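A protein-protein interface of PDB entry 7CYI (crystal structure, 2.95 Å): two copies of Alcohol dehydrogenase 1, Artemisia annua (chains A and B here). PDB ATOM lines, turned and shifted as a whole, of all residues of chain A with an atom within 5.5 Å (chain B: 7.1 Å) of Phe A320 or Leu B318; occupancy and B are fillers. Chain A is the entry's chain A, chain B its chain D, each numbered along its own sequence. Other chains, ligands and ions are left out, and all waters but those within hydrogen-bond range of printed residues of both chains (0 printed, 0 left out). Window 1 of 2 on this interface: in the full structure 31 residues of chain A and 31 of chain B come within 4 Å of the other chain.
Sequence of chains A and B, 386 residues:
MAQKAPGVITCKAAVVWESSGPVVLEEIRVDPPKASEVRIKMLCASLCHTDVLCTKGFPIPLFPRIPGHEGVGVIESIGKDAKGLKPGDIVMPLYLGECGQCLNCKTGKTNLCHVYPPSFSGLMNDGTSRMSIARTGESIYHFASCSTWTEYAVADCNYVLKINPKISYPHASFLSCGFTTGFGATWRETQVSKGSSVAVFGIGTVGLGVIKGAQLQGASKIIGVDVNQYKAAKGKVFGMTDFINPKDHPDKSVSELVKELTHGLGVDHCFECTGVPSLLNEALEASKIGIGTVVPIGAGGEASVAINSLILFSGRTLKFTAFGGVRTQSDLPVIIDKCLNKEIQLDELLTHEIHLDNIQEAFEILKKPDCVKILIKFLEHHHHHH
N of Phe B320 sits at hydrogen-bond distance from O of Arg A316 (3.0 Å).
The backbone NH of Leu B318 is in hydrogen-bond range of the backbone carbonyl oxygen of Leu A318.
NZ of Lys A319 lies within hydrogen-bond range of O of Gly B315.
The backbone NH (N) of Phe A320 sits at hydrogen-bond distance from the backbone carbonyl oxygen (O) of Arg B316, 3.0 Å away.
The backbone NH (N) of Thr A321 sits at hydrogen-bond distance from the backbone carbonyl oxygen (O) of Leu B312.
The side-chain carboxylate of Glu A189 lies within salt-bridge range of the side-chain amino group of Lys A319 (2.5 Å).
The side-chain carboxylate (OE2) of Glu A189 is in hydrogen-bond range of the side-chain hydroxyl (OG1) of Thr A321 (2.7 Å).
N of Lys A319 is in hydrogen-bond range of O of Val A294, at 3.0 Å.
O of Leu B284 is in hydrogen-bond range of NH1 of Arg B316, at 2.7 Å.
The backbone NH of Val B294 lies within hydrogen-bond range of the backbone carbonyl oxygen of Thr B317 (2.8 Å).
The side-chain hydroxyl (OG) of Ser B314 is in hydrogen-bond range of the backbone carbonyl oxygen (O) of Ile B311, 2.4 Å away.
Ile A307 touches Ile B307.
Lys B319 touches Arg A316 (C to O, 3.9 Å).
C of Thr A317 touches O of Leu B318, 3.8 Å away.
OG1 of Thr A317 touches CD of Lys B319 (3.5 Å).
Leu A318 touches Thr B317 (O to C, 3.7 Å).
Lys A319 touches Thr B317.
CD2 of Leu B284 touches CE2 of Phe A320, at 3.8 Å.
Ile B311 touches Phe A320 (O to CB, 3.5 Å).
O of Phe A320 touches CA of Gly B315, 3.1 Å away.
Thr A321 touches Phe B313 (O to CA, 3.2 Å).
Pro A296 touches none of the printed residues of chain B.
Printed residues of chain B within 4 Å of Arg A316: Leu B318, Lys B319 and Phe B320.
Of the printed residues of chain B, Thr A317 touches Leu B318 (3.8 Å) and Lys B319 (3.5 Å).
Of the printed residues of chain B, Leu A318 touches Thr B317, Leu B318 and Phe B320.
Of chain B, only Leu B284, Ile B311, Leu B312, Gly B315, Arg B316 and Leu B318 come within 4 Å of Phe A320.
Pro B296 touches none of the printed residues of chain A.
Of the printed residues of chain A, Ile B311 touches Phe A320 (3.5 Å).
Of the printed residues of chain A, Gly B315 touches Lys A319 (3.1 Å) and Phe A320 (3.1 Å).
Printed residues of chain A within 4 Å of Leu B318: Arg A316, Thr A317, Leu A318 and Phe A320.
The nearest printed residue of chain B that does not touch Leu A318 is Arg B316 (4.1 Å).
Hydrophobic or aromatic side chains of chain A that line the printed part of chain B: Ile A307, Leu A318, Phe A320 and Ala A322.
Of the 21 printed residues of chain B, 11 touch a printed residue of chain A.
Printed residues of chain B that touch a printed residue of chain A: Leu B284, Ile B307, Ile B311, Leu B312, Phe B313, Gly B315, Arg B316, Thr B317, Leu B318, Lys B319 and Phe B320.
Among the printed residues, no Asp or Glu carboxylate lies within 4 Å of a Lys or Arg side-chain nitrogen of the other chain.
Ile A307 touches its own counterpart, Ile B307.
Arg A316 touches Leu B318, but with the chains exchanged Leu A318 does not touch Arg B316 (4.1 Å).
Arg A316 touches Lys B319, and with the chains exchanged Lys A319 touches Arg B316.
Thr A317 touches Leu B318, and with the chains exchanged Leu A318 touches Thr B317.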
ATOM      1  N   GLU A 189      -9.395 -36.244  31.219  1.00  0.00           N
ATOM      2  CA  GLU A 189     -10.459 -35.359  30.755  1.00  0.00           C
ATOM      3  C   GLU A 189     -11.565 -36.101  30.015  1.00  0.00           C
ATOM      4  O   GLU A 189     -12.749 -35.859  30.269  1.00  0.00           O
ATOM      5  CB  GLU A 189      -9.876 -34.260  29.860  1.00  0.00           C
ATOM      6  CG  GLU A 189      -8.915 -33.325  30.571  1.00  0.00           C
ATOM      7  CD  GLU A 189      -9.602 -32.444  31.600  1.00  0.00           C
ATOM      8  OE1 GLU A 189     -10.850 -32.417  31.635  1.00  0.00           O
ATOM      9  OE2 GLU A 189      -8.891 -31.763  32.366  1.00  0.00           O
ATOM     10  N   VAL A 294     -15.289 -33.142  23.042  1.00  0.00           N
ATOM     11  CA  VAL A 294     -14.251 -32.261  22.521  1.00  0.00           C
ATOM     12  C   VAL A 294     -13.480 -31.672  23.694  1.00  0.00           C
ATOM     13  O   VAL A 294     -14.074 -31.278  24.704  1.00  0.00           O
ATOM     14  CB  VAL A 294     -14.846 -31.143  21.636  1.00  0.00           C
ATOM     15  CG1 VAL A 294     -13.752 -30.222  21.124  1.00  0.00           C
ATOM     16  CG2 VAL A 294     -15.623 -31.742  20.475  1.00  0.00           C
ATOM     17  N   PRO A 296     -10.735 -28.686  24.365  1.00  0.00           N
ATOM     18  CA  PRO A 296      -9.917 -27.582  23.849  1.00  0.00           C
ATOM     19  C   PRO A 296      -8.629 -27.398  24.638  1.00  0.00           C
ATOM     20  O   PRO A 296      -8.609 -26.723  25.672  1.00  0.00           O
ATOM     21  CB  PRO A 296     -10.844 -26.370  23.984  1.00  0.00           C
ATOM     22  CG  PRO A 296     -11.735 -26.714  25.128  1.00  0.00           C
ATOM     23  CD  PRO A 296     -11.904 -28.212  25.125  1.00  0.00           C
ATOM     24  N   ILE A 307     -18.792 -20.118  19.178  1.00  0.00           N
ATOM     25  CA  ILE A 307     -19.403 -21.433  19.024  1.00  0.00           C
ATOM     26  C   ILE A 307     -20.727 -21.263  18.295  1.00  0.00           C
ATOM     27  O   ILE A 307     -21.503 -20.353  18.606  1.00  0.00           O
ATOM     28  CB  ILE A 307     -19.615 -22.123  20.389  1.00  0.00           C
ATOM     29  CG1 ILE A 307     -18.270 -22.375  21.072  1.00  0.00           C
ATOM     30  CG2 ILE A 307     -20.390 -23.420  20.225  1.00  0.00           C
ATOM     31  CD1 ILE A 307     -18.386 -22.696  22.545  1.00  0.00           C
ATOM     32  N   ARG A 316     -23.358 -32.774  22.257  1.00  0.00           N
ATOM     33  CA  ARG A 316     -21.937 -33.033  22.423  1.00  0.00           C
ATOM     34  C   ARG A 316     -21.452 -32.542  23.784  1.00  0.00           C
ATOM     35  O   ARG A 316     -22.112 -31.751  24.463  1.00  0.00           O
ATOM     36  CB  ARG A 316     -21.140 -32.355  21.311  1.00  0.00           C
ATOM     37  CG  ARG A 316     -21.521 -32.804  19.915  1.00  0.00           C
ATOM     38  CD  ARG A 316     -20.870 -31.914  18.871  1.00  0.00           C
ATOM     39  NE  ARG A 316     -20.721 -32.590  17.586  1.00  0.00           N
ATOM     40  CZ  ARG A 316     -21.358 -32.242  16.473  1.00  0.00           C
ATOM     41  NH1 ARG A 316     -22.188 -31.210  16.474  1.00  0.00           N
ATOM     42  NH2 ARG A 316     -21.149 -32.918  15.353  1.00  0.00           N
ATOM     43  N   THR A 317     -20.272 -33.017  24.173  1.00  0.00           N
ATOM     44  CA  THR A 317     -19.655 -32.663  25.446  1.00  0.00           C
ATOM     45  C   THR A 317     -18.399 -31.848  25.180  1.00  0.00           C
ATOM     46  O   THR A 317     -17.506 -32.294  24.452  1.00  0.00           O
ATOM     47  CB  THR A 317     -19.316 -33.910  26.264  1.00  0.00           C
ATOM     48  OG1 THR A 317     -20.475 -34.745  26.374  1.00  0.00           O
ATOM     49  CG2 THR A 317     -18.846 -33.519  27.664  1.00  0.00           C
ATOM     50  N   LEU A 318     -18.334 -30.657  25.763  1.00  0.00           N
ATOM     51  CA  LEU A 318     -17.157 -29.800  25.694  1.00  0.00           C
ATOM     52  C   LEU A 318     -16.530 -29.782  27.081  1.00  0.00           C
ATOM     53  O   LEU A 318     -17.109 -29.226  28.020  1.00  0.00           O
ATOM     54  CB  LEU A 318     -17.528 -28.396  25.228  1.00  0.00           C
ATOM     55  CG  LEU A 318     -16.372 -27.425  24.991  1.00  0.00           C
ATOM     56  CD1 LEU A 318     -15.400 -27.982  23.966  1.00  0.00           C
ATOM     57  CD2 LEU A 318     -16.911 -26.080  24.545  1.00  0.00           C
ATOM     58  N   LYS A 319     -15.362 -30.402  27.214  1.00  0.00           N
ATOM     59  CA  LYS A 319     -14.687 -30.556  28.499  1.00  0.00           C
ATOM     60  C   LYS A 319     -13.459 -29.654  28.524  1.00  0.00           C
ATOM     61  O   LYS A 319     -12.468 -29.924  27.837  1.00  0.00           O
ATOM     62  CB  LYS A 319     -14.299 -32.013  28.742  1.00  0.00           C
ATOM     63  CG  LYS A 319     -13.708 -32.272  30.117  1.00  0.00           C
ATOM     64  CD  LYS A 319     -14.658 -31.818  31.213  1.00  0.00           C
ATOM     65  CE  LYS A 319     -14.157 -32.220  32.591  1.00  0.00           C
ATOM     66  NZ  LYS A 319     -12.821 -31.635  32.909  1.00  0.00           N
ATOM     67  N   PHE A 320     -13.524 -28.589  29.318  1.00  0.00           N
ATOM     68  CA  PHE A 320     -12.381 -27.706  29.470  1.00  0.00           C
ATOM     69  C   PHE A 320     -11.320 -28.364  30.350  1.00  0.00           C
ATOM     70  O   PHE A 320     -11.604 -29.257  31.154  1.00  0.00           O
ATOM     71  CB  PHE A 320     -12.821 -26.366  30.053  1.00  0.00           C
ATOM     72  CG  PHE A 320     -14.025 -25.784  29.373  1.00  0.00           C
ATOM     73  CD1 PHE A 320     -13.984 -25.444  28.031  1.00  0.00           C
ATOM     74  CD2 PHE A 320     -15.202 -25.586  30.070  1.00  0.00           C
ATOM     75  CE1 PHE A 320     -15.092 -24.914  27.401  1.00  0.00           C
ATOM     76  CE2 PHE A 320     -16.314 -25.053  29.445  1.00  0.00           C
ATOM     77  CZ  PHE A 320     -16.257 -24.717  28.109  1.00  0.00           C
ATOM     78  N   THR A 321     -10.076 -27.920  30.182  1.00  0.00           N
ATOM     79  CA  THR A 321      -8.957 -28.613  30.800  1.00  0.00           C
ATOM     80  C   THR A 321      -7.837 -27.630  31.099  1.00  0.00           C
ATOM     81  O   THR A 321      -7.756 -26.547  30.514  1.00  0.00           O
ATOM     82  CB  THR A 321      -8.437 -29.742  29.902  1.00  0.00           C
ATOM     83  OG1 THR A 321      -7.374 -30.434  30.567  1.00  0.00           O
ATOM     84  CG2 THR A 321      -7.924 -29.185  28.584  1.00  0.00           C
ATOM     85  N   ALA A 322      -6.970 -28.030  32.026  1.00  0.00           N
ATOM     86  CA  ALA A 322      -5.751 -27.300  32.341  1.00  0.00           C
ATOM     87  C   ALA A 322      -4.676 -28.316  32.683  1.00  0.00           C
ATOM     88  O   ALA A 322      -4.881 -29.159  33.560  1.00  0.00           O
ATOM     89  CB  ALA A 322      -5.960 -26.325  33.503  1.00  0.00           C
ATOM     90  N   LEU B 280     -24.720 -17.326  29.355  1.00  0.00           N
ATOM     91  CA  LEU B 280     -23.970 -18.578  29.345  1.00  0.00           C
ATOM     92  C   LEU B 280     -22.579 -18.387  29.939  1.00  0.00           C
ATOM     93  O   LEU B 280     -22.063 -19.277  30.625  1.00  0.00           O
ATOM     94  CB  LEU B 280     -23.881 -19.148  27.928  1.00  0.00           C
ATOM     95  CG  LEU B 280     -22.948 -20.357  27.815  1.00  0.00           C
ATOM     96  CD1 LEU B 280     -23.711 -21.652  28.007  1.00  0.00           C
ATOM     97  CD2 LEU B 280     -22.216 -20.367  26.493  1.00  0.00           C
ATOM     98  N   LEU B 284     -21.187 -20.338  33.335  1.00  0.00           N
ATOM     99  CA  LEU B 284     -19.917 -21.038  33.489  1.00  0.00           C
ATOM    100  C   LEU B 284     -19.185 -20.574  34.742  1.00  0.00           C
ATOM    101  O   LEU B 284     -18.714 -21.395  35.537  1.00  0.00           O
ATOM    102  CB  LEU B 284     -19.054 -20.837  32.242  1.00  0.00           C
ATOM    103  CG  LEU B 284     -19.487 -21.607  30.993  1.00  0.00           C
ATOM    104  CD1 LEU B 284     -18.844 -21.016  29.749  1.00  0.00           C
ATOM    105  CD2 LEU B 284     -19.142 -23.082  31.124  1.00  0.00           C
ATOM    106  N   GLY B 290     -13.374 -26.743  38.186  1.00  0.00           N
ATOM    107  CA  GLY B 290     -12.864 -28.099  38.126  1.00  0.00           C
ATOM    108  C   GLY B 290     -13.926 -29.175  38.044  1.00  0.00           C
ATOM    109  O   GLY B 290     -13.758 -30.160  37.317  1.00  0.00           O
ATOM    110  N   GLY B 292     -17.514 -28.184  38.037  1.00  0.00           N
ATOM    111  CA  GLY B 292     -18.785 -27.615  37.645  1.00  0.00           C
ATOM    112  C   GLY B 292     -19.253 -28.105  36.286  1.00  0.00           C
ATOM    113  O   GLY B 292     -18.476 -28.575  35.456  1.00  0.00           O
ATOM    114  N   THR B 293     -20.559 -27.982  36.060  1.00  0.00           N
ATOM    115  CA  THR B 293     -21.184 -28.423  34.822  1.00  0.00           C
ATOM    116  C   THR B 293     -22.248 -27.416  34.414  1.00  0.00           C
ATOM    117  O   THR B 293     -22.988 -26.911  35.261  1.00  0.00           O
ATOM    118  CB  THR B 293     -21.815 -29.815  34.976  1.00  0.00           C
ATOM    119  OG1 THR B 293     -20.907 -30.681  35.669  1.00  0.00           O
ATOM    120  CG2 THR B 293     -22.136 -30.416  33.614  1.00  0.00           C
ATOM    121  N   VAL B 294     -22.327 -27.129  33.117  1.00  0.00           N
ATOM    122  CA  VAL B 294     -23.279 -26.162  32.585  1.00  0.00           C
ATOM    123  C   VAL B 294     -24.079 -26.824  31.473  1.00  0.00           C
ATOM    124  O   VAL B 294     -23.506 -27.447  30.573  1.00  0.00           O
ATOM    125  CB  VAL B 294     -22.576 -24.891  32.073  1.00  0.00           C
ATOM    126  CG1 VAL B 294     -23.565 -23.975  31.381  1.00  0.00           C
ATOM    127  CG2 VAL B 294     -21.897 -24.170  33.224  1.00  0.00           C
ATOM    128  N   VAL B 295     -25.397 -26.694  31.536  1.00  0.00           N
ATOM    129  CA  VAL B 295     -26.301 -27.250  30.543  1.00  0.00           C
ATOM    130  C   VAL B 295     -27.036 -26.098  29.869  1.00  0.00           C
ATOM    131  O   VAL B 295     -28.027 -25.586  30.391  1.00  0.00           O
ATOM    132  CB  VAL B 295     -27.292 -28.241  31.180  1.00  0.00           C
ATOM    133  CG1 VAL B 295     -28.233 -28.802  30.134  1.00  0.00           C
ATOM    134  CG2 VAL B 295     -26.542 -29.363  31.872  1.00  0.00           C
ATOM    135  N   PRO B 296     -26.570 -25.651  28.700  1.00  0.00           N
ATOM    136  CA  PRO B 296     -27.257 -24.556  28.000  1.00  0.00           C
ATOM    137  C   PRO B 296     -28.550 -25.011  27.345  1.00  0.00           C
ATOM    138  O   PRO B 296     -28.545 -25.502  26.210  1.00  0.00           O
ATOM    139  CB  PRO B 296     -26.223 -24.103  26.962  1.00  0.00           C
ATOM    140  CG  PRO B 296     -25.395 -25.314  26.708  1.00  0.00           C
ATOM    141  CD  PRO B 296     -25.332 -26.059  28.013  1.00  0.00           C
ATOM    142  N   ILE B 307     -17.694 -17.239  24.542  1.00  0.00           N
ATOM    143  CA  ILE B 307     -17.298 -17.720  25.858  1.00  0.00           C
ATOM    144  C   ILE B 307     -15.929 -17.142  26.188  1.00  0.00           C
ATOM    145  O   ILE B 307     -15.049 -17.084  25.323  1.00  0.00           O
ATOM    146  CB  ILE B 307     -17.272 -19.262  25.908  1.00  0.00           C
ATOM    147  CG1 ILE B 307     -18.693 -19.822  25.862  1.00  0.00           C
ATOM    148  CG2 ILE B 307     -16.555 -19.760  27.153  1.00  0.00           C
ATOM    149  CD1 ILE B 307     -18.745 -21.331  25.928  1.00  0.00           C
ATOM    150  N   ASN B 308     -15.759 -16.701  27.435  1.00  0.00           N
ATOM    151  CA  ASN B 308     -14.469 -16.207  27.902  1.00  0.00           C
ATOM    152  C   ASN B 308     -13.377 -17.243  27.659  1.00  0.00           C
ATOM    153  O   ASN B 308     -13.516 -18.413  28.030  1.00  0.00           O
ATOM    154  CB  ASN B 308     -14.555 -15.860  29.391  1.00  0.00           C
ATOM    155  CG  ASN B 308     -13.485 -14.876  29.829  1.00  0.00           C
ATOM    156  OD1 ASN B 308     -12.376 -14.862  29.289  1.00  0.00           O
ATOM    157  ND2 ASN B 308     -13.813 -14.046  30.817  1.00  0.00           N
ATOM    158  N   LEU B 310     -10.539 -17.728  28.961  1.00  0.00           N
ATOM    159  CA  LEU B 310      -9.905 -18.303  30.141  1.00  0.00           C
ATOM    160  C   LEU B 310     -10.746 -19.390  30.796  1.00  0.00           C
ATOM    161  O   LEU B 310     -10.232 -20.116  31.654  1.00  0.00           O
ATOM    162  CB  LEU B 310      -9.592 -17.201  31.156  1.00  0.00           C
ATOM    163  CG  LEU B 310      -8.528 -16.198  30.700  1.00  0.00           C
ATOM    164  CD1 LEU B 310      -8.187 -15.220  31.814  1.00  0.00           C
ATOM    165  CD2 LEU B 310      -7.279 -16.919  30.207  1.00  0.00           C
ATOM    166  N   ILE B 311     -12.018 -19.517  30.412  1.00  0.00           N
ATOM    167  CA  ILE B 311     -12.843 -20.603  30.926  1.00  0.00           C
ATOM    168  C   ILE B 311     -12.368 -21.939  30.370  1.00  0.00           C
ATOM    169  O   ILE B 311     -12.552 -22.987  31.005  1.00  0.00           O
ATOM    170  CB  ILE B 311     -14.323 -20.332  30.603  1.00  0.00           C
ATOM    171  CG1 ILE B 311     -14.755 -18.999  31.212  1.00  0.00           C
ATOM    172  CG2 ILE B 311     -15.214 -21.445  31.124  1.00  0.00           C
ATOM    173  CD1 ILE B 311     -16.223 -18.692  31.034  1.00  0.00           C
ATOM    174  N   LEU B 312     -11.724 -21.930  29.198  1.00  0.00           N
ATOM    175  CA  LEU B 312     -11.178 -23.153  28.621  1.00  0.00           C
ATOM    176  C   LEU B 312     -10.105 -23.784  29.498  1.00  0.00           C
ATOM    177  O   LEU B 312      -9.722 -24.932  29.247  1.00  0.00           O
ATOM    178  CB  LEU B 312     -10.603 -22.879  27.228  1.00  0.00           C
ATOM    179  CG  LEU B 312     -11.452 -22.113  26.206  1.00  0.00           C
ATOM    180  CD1 LEU B 312     -10.861 -22.249  24.809  1.00  0.00           C
ATOM    181  CD2 LEU B 312     -12.895 -22.573  26.214  1.00  0.00           C
ATOM    182  N   PHE B 313      -9.615 -23.070  30.509  1.00  0.00           N
ATOM    183  CA  PHE B 313      -8.664 -23.601  31.476  1.00  0.00           C
ATOM    184  C   PHE B 313      -9.315 -23.973  32.805  1.00  0.00           C
ATOM    185  O   PHE B 313      -8.619 -24.449  33.707  1.00  0.00           O
ATOM    186  CB  PHE B 313      -7.540 -22.586  31.730  1.00  0.00           C
ATOM    187  CG  PHE B 313      -6.761 -22.207  30.499  1.00  0.00           C
ATOM    188  CD1 PHE B 313      -5.564 -22.835  30.203  1.00  0.00           C
ATOM    189  CD2 PHE B 313      -7.216 -21.211  29.651  1.00  0.00           C
ATOM    190  CE1 PHE B 313      -4.842 -22.487  29.076  1.00  0.00           C
ATOM    191  CE2 PHE B 313      -6.497 -20.859  28.523  1.00  0.00           C
ATOM    192  CZ  PHE B 313      -5.308 -21.499  28.237  1.00  0.00           C
ATOM    193  N   SER B 314     -10.626 -23.771  32.947  1.00  0.00           N
ATOM    194  CA  SER B 314     -11.300 -23.931  34.230  1.00  0.00           C
ATOM    195  C   SER B 314     -11.723 -25.365  34.523  1.00  0.00           C
ATOM    196  O   SER B 314     -12.219 -25.633  35.623  1.00  0.00           O
ATOM    197  CB  SER B 314     -12.530 -23.018  34.296  1.00  0.00           C
ATOM    198  OG  SER B 314     -13.433 -23.291  33.237  1.00  0.00           O
ATOM    199  N   GLY B 315     -11.555 -26.283  33.576  1.00  0.00           N
ATOM    200  CA  GLY B 315     -11.869 -27.675  33.824  1.00  0.00           C
ATOM    201  C   GLY B 315     -13.336 -27.999  33.997  1.00  0.00           C
ATOM    202  O   GLY B 315     -13.659 -29.109  34.433  1.00  0.00           O
ATOM    203  N   ARG B 316     -14.236 -27.075  33.671  1.00  0.00           N
ATOM    204  CA  ARG B 316     -15.664 -27.329  33.794  1.00  0.00           C
ATOM    205  C   ARG B 316     -16.146 -28.207  32.643  1.00  0.00           C
ATOM    206  O   ARG B 316     -15.396 -28.545  31.721  1.00  0.00           O
ATOM    207  CB  ARG B 316     -16.442 -26.016  33.832  1.00  0.00           C
ATOM    208  CG  ARG B 316     -15.857 -24.965  34.750  1.00  0.00           C
ATOM    209  CD  ARG B 316     -16.583 -23.647  34.579  1.00  0.00           C
ATOM    210  NE  ARG B 316     -15.752 -22.507  34.954  1.00  0.00           N
ATOM    211  CZ  ARG B 316     -15.805 -21.897  36.133  1.00  0.00           C
ATOM    212  NH1 ARG B 316     -16.653 -22.317  37.062  1.00  0.00           N
ATOM    213  NH2 ARG B 316     -15.016 -20.863  36.383  1.00  0.00           N
ATOM    214  N   THR B 317     -17.423 -28.575  32.691  1.00  0.00           N
ATOM    215  CA  THR B 317     -18.046 -29.413  31.673  1.00  0.00           C
ATOM    216  C   THR B 317     -19.199 -28.648  31.042  1.00  0.00           C
ATOM    217  O   THR B 317     -20.111 -28.201  31.744  1.00  0.00           O
ATOM    218  CB  THR B 317     -18.542 -30.732  32.269  1.00  0.00           C
ATOM    219  OG1 THR B 317     -17.438 -31.448  32.837  1.00  0.00           O
ATOM    220  CG2 THR B 317     -19.198 -31.588  31.195  1.00  0.00           C
ATOM    221  N   LEU B 318     -19.158 -28.504  29.724  1.00  0.00           N
ATOM    222  CA  LEU B 318     -20.209 -27.833  28.963  1.00  0.00           C
ATOM    223  C   LEU B 318     -20.949 -28.903  28.167  1.00  0.00           C
ATOM    224  O   LEU B 318     -20.474 -29.355  27.122  1.00  0.00           O
ATOM    225  CB  LEU B 318     -19.622 -26.756  28.060  1.00  0.00           C
ATOM    226  CG  LEU B 318     -20.635 -25.835  27.390  1.00  0.00           C
ATOM    227  CD1 LEU B 318     -21.546 -25.221  28.433  1.00  0.00           C
ATOM    228  CD2 LEU B 318     -19.911 -24.757  26.607  1.00  0.00           C
ATOM    229  N   LYS B 319     -22.111 -29.309  28.672  1.00  0.00           N
ATOM    230  CA  LYS B 319     -22.892 -30.400  28.094  1.00  0.00           C
ATOM    231  C   LYS B 319     -24.005 -29.795  27.248  1.00  0.00           C
ATOM    232  O   LYS B 319     -24.999 -29.292  27.775  1.00  0.00           O
ATOM    233  CB  LYS B 319     -23.451 -31.302  29.192  1.00  0.00           C
ATOM    234  CG  LYS B 319     -24.202 -32.525  28.684  1.00  0.00           C
ATOM    235  CD  LYS B 319     -23.266 -33.508  27.999  1.00  0.00           C
ATOM    236  CE  LYS B 319     -24.013 -34.744  27.522  1.00  0.00           C
ATOM    237  NZ  LYS B 319     -25.037 -34.415  26.493  1.00  0.00           N
ATOM    238  N   PHE B 320     -23.836 -29.846  25.931  1.00  0.00           N
ATOM    239  CA  PHE B 320     -24.884 -29.380  25.037  1.00  0.00           C
ATOM    240  C   PHE B 320     -26.045 -30.369  25.032  1.00  0.00           C
ATOM    241  O   PHE B 320     -25.876 -31.560  25.306  1.00  0.00           O
ATOM    242  CB  PHE B 320     -24.327 -29.178  23.630  1.00  0.00           C
ATOM    243  CG  PHE B 320     -23.101 -28.311  23.591  1.00  0.00           C
ATOM    244  CD1 PHE B 320     -23.176 -26.970  23.927  1.00  0.00           C
ATOM    245  CD2 PHE B 320     -21.873 -28.839  23.233  1.00  0.00           C
ATOM    246  CE1 PHE B 320     -22.053 -26.171  23.899  1.00  0.00           C
ATOM    247  CE2 PHE B 320     -20.745 -28.043  23.202  1.00  0.00           C
ATOM    248  CZ  PHE B 320     -20.837 -26.707  23.535  1.00  0.00           C
